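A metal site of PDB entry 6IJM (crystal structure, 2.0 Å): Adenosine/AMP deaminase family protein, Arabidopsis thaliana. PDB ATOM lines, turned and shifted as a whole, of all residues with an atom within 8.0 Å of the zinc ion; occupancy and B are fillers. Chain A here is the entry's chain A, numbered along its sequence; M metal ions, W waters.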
ATOM      1  N   HIS A  34      15.346 -22.696 -22.629  1.00  0.00           N
ATOM      2  CA  HIS A  34      16.339 -23.520 -21.936  1.00  0.00           C
ATOM      3  C   HIS A  34      17.716 -23.031 -22.359  1.00  0.00           C
ATOM      4  O   HIS A  34      18.315 -23.551 -23.308  1.00  0.00           O
ATOM      5  CB  HIS A  34      16.127 -25.007 -22.212  1.00  0.00           C
ATOM      6  CG  HIS A  34      16.938 -25.939 -21.361  1.00  0.00           C
ATOM      7  ND1 HIS A  34      16.420 -27.101 -20.837  1.00  0.00           N
ATOM      8  CD2 HIS A  34      18.250 -25.925 -21.001  1.00  0.00           C
ATOM      9  CE1 HIS A  34      17.373 -27.742 -20.165  1.00  0.00           C
ATOM     10  NE2 HIS A  34      18.498 -27.055 -20.259  1.00  0.00           N
ATOM     11  N   ALA A  35      18.218 -22.037 -21.648  1.00  0.00           N
ATOM     12  CA  ALA A  35      19.542 -21.475 -21.911  1.00  0.00           C
ATOM     13  C   ALA A  35      20.184 -21.179 -20.581  1.00  0.00           C
ATOM     14  O   ALA A  35      19.619 -20.422 -19.785  1.00  0.00           O
ATOM     15  CB  ALA A  35      19.446 -20.205 -22.775  1.00  0.00           C
ATOM     16  N   HIS A  36      21.349 -21.774 -20.335  1.00  0.00           N
ATOM     17  CA  HIS A  36      22.096 -21.576 -19.109  1.00  0.00           C
ATOM     18  C   HIS A  36      23.018 -20.371 -19.248  1.00  0.00           C
ATOM     19  O   HIS A  36      23.670 -20.195 -20.288  1.00  0.00           O
ATOM     20  CB  HIS A  36      22.937 -22.826 -18.757  1.00  0.00           C
ATOM     21  CG  HIS A  36      22.133 -24.067 -18.496  1.00  0.00           C
ATOM     22  ND1 HIS A  36      21.706 -24.430 -17.241  1.00  0.00           N
ATOM     23  CD2 HIS A  36      21.718 -25.054 -19.331  1.00  0.00           C
ATOM     24  CE1 HIS A  36      21.066 -25.584 -17.303  1.00  0.00           C
ATOM     25  NE2 HIS A  36      21.047 -25.986 -18.559  1.00  0.00           N
ATOM     26  N   PHE A  82      33.165 -26.490 -19.425  1.00  0.00           N
ATOM     27  CA  PHE A  82      32.327 -26.430 -18.228  1.00  0.00           C
ATOM     28  C   PHE A  82      33.184 -26.286 -16.972  1.00  0.00           C
ATOM     29  O   PHE A  82      32.947 -25.408 -16.119  1.00  0.00           O
ATOM     30  CB  PHE A  82      31.434 -27.664 -18.161  1.00  0.00           C
ATOM     31  CG  PHE A  82      30.286 -27.641 -19.139  1.00  0.00           C
ATOM     32  CD1 PHE A  82      29.520 -26.491 -19.301  1.00  0.00           C
ATOM     33  CD2 PHE A  82      29.982 -28.745 -19.921  1.00  0.00           C
ATOM     34  CE1 PHE A  82      28.465 -26.441 -20.202  1.00  0.00           C
ATOM     35  CE2 PHE A  82      28.928 -28.709 -20.842  1.00  0.00           C
ATOM     36  CZ  PHE A  82      28.165 -27.558 -20.980  1.00  0.00           C
ATOM     37  N   ARG A 117      18.306 -19.265 -17.211  1.00  0.00           N
ATOM     38  CA  ARG A 117      18.423 -20.032 -15.983  1.00  0.00           C
ATOM     39  C   ARG A 117      19.854 -19.984 -15.484  1.00  0.00           C
ATOM     40  O   ARG A 117      20.803 -19.986 -16.266  1.00  0.00           O
ATOM     41  CB  ARG A 117      17.973 -21.493 -16.158  1.00  0.00           C
ATOM     42  CG  ARG A 117      18.784 -22.349 -17.118  1.00  0.00           C
ATOM     43  CD  ARG A 117      18.097 -23.732 -17.327  1.00  0.00           C
ATOM     44  NE  ARG A 117      16.820 -23.670 -18.067  1.00  0.00           N
ATOM     45  CZ  ARG A 117      15.941 -24.674 -18.129  1.00  0.00           C
ATOM     46  NH1 ARG A 117      16.180 -25.822 -17.480  1.00  0.00           N
ATOM     47  NH2 ARG A 117      14.821 -24.534 -18.828  1.00  0.00           N
ATOM     48  N   SER A 179      18.144 -22.359 -10.895  1.00  0.00           N
ATOM     49  CA  SER A 179      18.376 -23.792 -10.965  1.00  0.00           C
ATOM     50  C   SER A 179      18.901 -24.300  -9.636  1.00  0.00           C
ATOM     51  O   SER A 179      19.801 -23.691  -9.049  1.00  0.00           O
ATOM     52  CB  SER A 179      19.402 -24.157 -12.052  1.00  0.00           C
ATOM     53  OG  SER A 179      18.924 -23.920 -13.353  1.00  0.00           O
ATOM     54  N   ASP A 208      14.335 -24.520 -11.716  1.00  0.00           N
ATOM     55  CA  ASP A 208      14.819 -25.609 -12.550  1.00  0.00           C
ATOM     56  C   ASP A 208      15.562 -26.630 -11.678  1.00  0.00           C
ATOM     57  O   ASP A 208      16.074 -26.290 -10.601  1.00  0.00           O
ATOM     58  CB  ASP A 208      15.749 -25.052 -13.643  1.00  0.00           C
ATOM     59  CG  ASP A 208      16.435 -26.124 -14.456  1.00  0.00           C
ATOM     60  OD1 ASP A 208      15.817 -27.164 -14.794  1.00  0.00           O
ATOM     61  OD2 ASP A 208      17.635 -25.908 -14.771  1.00  0.00           O
ATOM     62  N   LEU A 209      15.590 -27.881 -12.121  1.00  0.00           N
ATOM     63  CA  LEU A 209      16.518 -28.864 -11.531  1.00  0.00           C
ATOM     64  C   LEU A 209      17.491 -29.324 -12.611  1.00  0.00           C
ATOM     65  O   LEU A 209      17.077 -29.836 -13.652  1.00  0.00           O
ATOM     66  CB  LEU A 209      15.798 -30.085 -10.944  1.00  0.00           C
ATOM     67  CG  LEU A 209      16.749 -31.145 -10.300  1.00  0.00           C
ATOM     68  CD1 LEU A 209      17.411 -30.602  -9.030  1.00  0.00           C
ATOM     69  CD2 LEU A 209      16.098 -32.486 -10.009  1.00  0.00           C
ATOM     70  N   SER A 210      18.796 -29.141 -12.353  1.00  0.00           N
ATOM     71  CA  SER A 210      19.822 -29.418 -13.363  1.00  0.00           C
ATOM     72  C   SER A 210      21.098 -29.922 -12.675  1.00  0.00           C
ATOM     73  O   SER A 210      21.156 -30.109 -11.460  1.00  0.00           O
ATOM     74  CB  SER A 210      20.117 -28.171 -14.200  1.00  0.00           C
ATOM     75  OG  SER A 210      20.786 -27.196 -13.419  1.00  0.00           O
ATOM     76  N   GLY A 211      22.131 -30.106 -13.480  1.00  0.00           N
ATOM     77  CA  GLY A 211      23.387 -30.656 -13.005  1.00  0.00           C
ATOM     78  C   GLY A 211      23.581 -32.067 -13.545  1.00  0.00           C
ATOM     79  O   GLY A 211      22.848 -32.529 -14.417  1.00  0.00           O
ATOM     80  N   HIS A 238      15.182 -30.801 -15.725  1.00  0.00           N
ATOM     81  CA  HIS A 238      16.009 -31.648 -16.601  1.00  0.00           C
ATOM     82  C   HIS A 238      15.617 -33.109 -16.363  1.00  0.00           C
ATOM     83  O   HIS A 238      15.723 -33.609 -15.242  1.00  0.00           O
ATOM     84  CB  HIS A 238      17.512 -31.462 -16.312  1.00  0.00           C
ATOM     85  CG  HIS A 238      18.143 -30.234 -16.924  1.00  0.00           C
ATOM     86  ND1 HIS A 238      17.861 -28.954 -16.498  1.00  0.00           N
ATOM     87  CD2 HIS A 238      19.092 -30.114 -17.886  1.00  0.00           C
ATOM     88  CE1 HIS A 238      18.586 -28.092 -17.183  1.00  0.00           C
ATOM     89  NE2 HIS A 238      19.361 -28.765 -18.023  1.00  0.00           N
ATOM     90  N   GLU A 241      17.768 -37.409 -18.914  1.00  0.00           N
ATOM     91  CA  GLU A 241      19.045 -37.258 -19.612  1.00  0.00           C
ATOM     92  C   GLU A 241      19.853 -38.546 -19.605  1.00  0.00           C
ATOM     93  O   GLU A 241      20.722 -38.727 -20.462  1.00  0.00           O
ATOM     94  CB  GLU A 241      19.872 -36.134 -18.979  1.00  0.00           C
ATOM     95  CG  GLU A 241      19.231 -34.765 -19.042  1.00  0.00           C
ATOM     96  CD  GLU A 241      20.020 -33.724 -18.264  1.00  0.00           C
ATOM     97  OE1 GLU A 241      20.725 -32.933 -18.901  1.00  0.00           O
ATOM     98  OE2 GLU A 241      19.927 -33.719 -17.014  1.00  0.00           O
ATOM     99  N   GLY A 260      12.966 -30.641 -19.582  1.00  0.00           N
ATOM    100  CA  GLY A 260      14.047 -30.562 -20.551  1.00  0.00           C
ATOM    101  C   GLY A 260      14.475 -31.954 -20.999  1.00  0.00           C
ATOM    102  O   GLY A 260      14.641 -32.870 -20.183  1.00  0.00           O
ATOM    103  N   HIS A 261      14.605 -32.102 -22.337  1.00  0.00           N
ATOM    104  CA  HIS A 261      15.284 -33.213 -23.018  1.00  0.00           C
ATOM    105  C   HIS A 261      14.418 -34.450 -23.232  1.00  0.00           C
ATOM    106  O   HIS A 261      14.006 -34.715 -24.359  1.00  0.00           O
ATOM    107  CB  HIS A 261      16.579 -33.595 -22.289  1.00  0.00           C
ATOM    108  CG  HIS A 261      17.501 -32.438 -22.046  1.00  0.00           C
ATOM    109  ND1 HIS A 261      18.027 -31.688 -23.070  1.00  0.00           N
ATOM    110  CD2 HIS A 261      17.972 -31.899 -20.891  1.00  0.00           C
ATOM    111  CE1 HIS A 261      18.791 -30.737 -22.561  1.00  0.00           C
ATOM    112  NE2 HIS A 261      18.771 -30.839 -21.241  1.00  0.00           N
ATOM    113  N   GLU A 281      11.297 -28.999 -23.595  1.00  0.00           N
ATOM    114  CA  GLU A 281      12.377 -28.179 -24.144  1.00  0.00           C
ATOM    115  C   GLU A 281      13.330 -29.095 -24.893  1.00  0.00           C
ATOM    116  O   GLU A 281      13.993 -29.937 -24.274  1.00  0.00           O
ATOM    117  CB  GLU A 281      13.093 -27.440 -23.007  1.00  0.00           C
ATOM    118  CG  GLU A 281      12.179 -26.643 -22.092  1.00  0.00           C
ATOM    119  CD  GLU A 281      12.659 -26.543 -20.631  1.00  0.00           C
ATOM    120  OE1 GLU A 281      13.706 -27.132 -20.288  1.00  0.00           O
ATOM    121  OE2 GLU A 281      11.988 -25.854 -19.831  1.00  0.00           O
ATOM    122  N   CYS A 283      16.637 -29.753 -27.045  1.00  0.00           N
ATOM    123  CA  CYS A 283      17.988 -29.212 -27.232  1.00  0.00           C
ATOM    124  C   CYS A 283      18.720 -30.101 -28.229  1.00  0.00           C
ATOM    125  O   CYS A 283      19.454 -31.014 -27.836  1.00  0.00           O
ATOM    126  CB  CYS A 283      18.692 -29.145 -25.878  1.00  0.00           C
ATOM    127  SG  CYS A 283      17.770 -28.173 -24.633  1.00  0.00           S
ATOM    128  N   SER A 286      22.782 -30.015 -28.335  1.00  0.00           N
ATOM    129  CA  SER A 286      23.185 -30.536 -27.030  1.00  0.00           C
ATOM    130  C   SER A 286      23.023 -32.064 -26.955  1.00  0.00           C
ATOM    131  O   SER A 286      23.980 -32.786 -26.634  1.00  0.00           O
ATOM    132  CB  SER A 286      22.368 -29.850 -25.933  1.00  0.00           C
ATOM    133  OG  SER A 286      22.788 -30.305 -24.663  1.00  0.00           O
ATOM    134  N   THR A 315      18.577 -23.778 -26.981  1.00  0.00           N
ATOM    135  CA  THR A 315      20.015 -23.922 -27.194  1.00  0.00           C
ATOM    136  C   THR A 315      20.715 -24.758 -26.120  1.00  0.00           C
ATOM    137  O   THR A 315      21.663 -25.478 -26.453  1.00  0.00           O
ATOM    138  CB  THR A 315      20.697 -22.542 -27.257  1.00  0.00           C
ATOM    139  OG1 THR A 315      20.385 -21.791 -26.082  1.00  0.00           O
ATOM    140  CG2 THR A 315      20.244 -21.760 -28.502  1.00  0.00           C
ATOM    141  N   ASP A 316      20.275 -24.674 -24.853  1.00  0.00           N
ATOM    142  CA  ASP A 316      20.915 -25.281 -23.687  1.00  0.00           C
ATOM    143  C   ASP A 316      22.213 -24.543 -23.308  1.00  0.00           C
ATOM    144  O   ASP A 316      22.261 -23.839 -22.290  1.00  0.00           O
ATOM    145  CB  ASP A 316      21.159 -26.780 -23.923  1.00  0.00           C
ATOM    146  CG  ASP A 316      21.331 -27.581 -22.619  1.00  0.00           C
ATOM    147  OD1 ASP A 316      21.130 -27.021 -21.503  1.00  0.00           O
ATOM    148  OD2 ASP A 316      21.638 -28.785 -22.743  1.00  0.00           O
ATOM    149  N   ASP A 317      23.280 -24.689 -24.107  1.00  0.00           N
ATOM    150  CA  ASP A 317      24.532 -23.935 -23.871  1.00  0.00           C
ATOM    151  C   ASP A 317      25.086 -23.530 -25.236  1.00  0.00           C
ATOM    152  O   ASP A 317      25.904 -24.243 -25.812  1.00  0.00           O
ATOM    153  CB  ASP A 317      25.568 -24.763 -23.093  1.00  0.00           C
ATOM    154  CG  ASP A 317      25.028 -25.297 -21.756  1.00  0.00           C
ATOM    155  OD1 ASP A 317      24.988 -24.551 -20.774  1.00  0.00           O
ATOM    156  OD2 ASP A 317      24.654 -26.475 -21.704  1.00  0.00           O
ATOM    157  N   PHE A 321      28.357 -25.221 -26.976  1.00  0.00           N
ATOM    158  CA  PHE A 321      28.054 -26.125 -28.086  1.00  0.00           C
ATOM    159  C   PHE A 321      28.218 -25.487 -29.464  1.00  0.00           C
ATOM    160  O   PHE A 321      27.925 -26.128 -30.477  1.00  0.00           O
ATOM    161  CB  PHE A 321      26.626 -26.689 -27.932  1.00  0.00           C
ATOM    162  CG  PHE A 321      26.486 -27.661 -26.784  1.00  0.00           C
ATOM    163  CD1 PHE A 321      27.149 -28.883 -26.802  1.00  0.00           C
ATOM    164  CD2 PHE A 321      25.699 -27.341 -25.689  1.00  0.00           C
ATOM    165  CE1 PHE A 321      27.018 -29.765 -25.750  1.00  0.00           C
ATOM    166  CE2 PHE A 321      25.573 -28.226 -24.629  1.00  0.00           C
ATOM    167  CZ  PHE A 321      26.239 -29.444 -24.660  1.00  0.00           C
HETATM  168 ZN    ZN M   1      20.464 -27.779 -19.607  1.00  0.00          ZN
HETATM  169  O   HOH W   1      20.792 -29.748 -20.577  1.00  0.00           O
HETATM  170  O   HOH W   2      22.609 -28.678 -19.130  1.00  0.00           O
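The side-chain carboxylate (OD2) of Asp 316 lies within hydrogen-bond range of the side-chain hydroxyl (OG) of Ser 286 (2.7 Å). The side-chain carboxylate of Asp 208 lies within hydrogen-bond range of a ring nitrogen (ND1) of His 238 (3.2 Å). The backbone NH (N) of His 238 lies within hydrogen-bond range of the backbone carbonyl oxygen (O) of Leu 209. The side-chain carboxylate (OE1) of Glu 281 lies within hydrogen-bond range of a ring nitrogen (ND1) of His 34 (2.8 Å). The backbone NH of His 261 sits at hydrogen-bond distance from the backbone carbonyl oxygen of Glu 281 (3.0 Å).
NE2 of His 261 touches the zinc ion (3.9 Å). Of the 21 residues printed, 5 come within 4 Å of the zinc ion.
The zinc ion is bound by OD1 of Asp 316, NE2 of His 36, NE2 of His 238, NE2 of His 34, water W1 and water W2.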
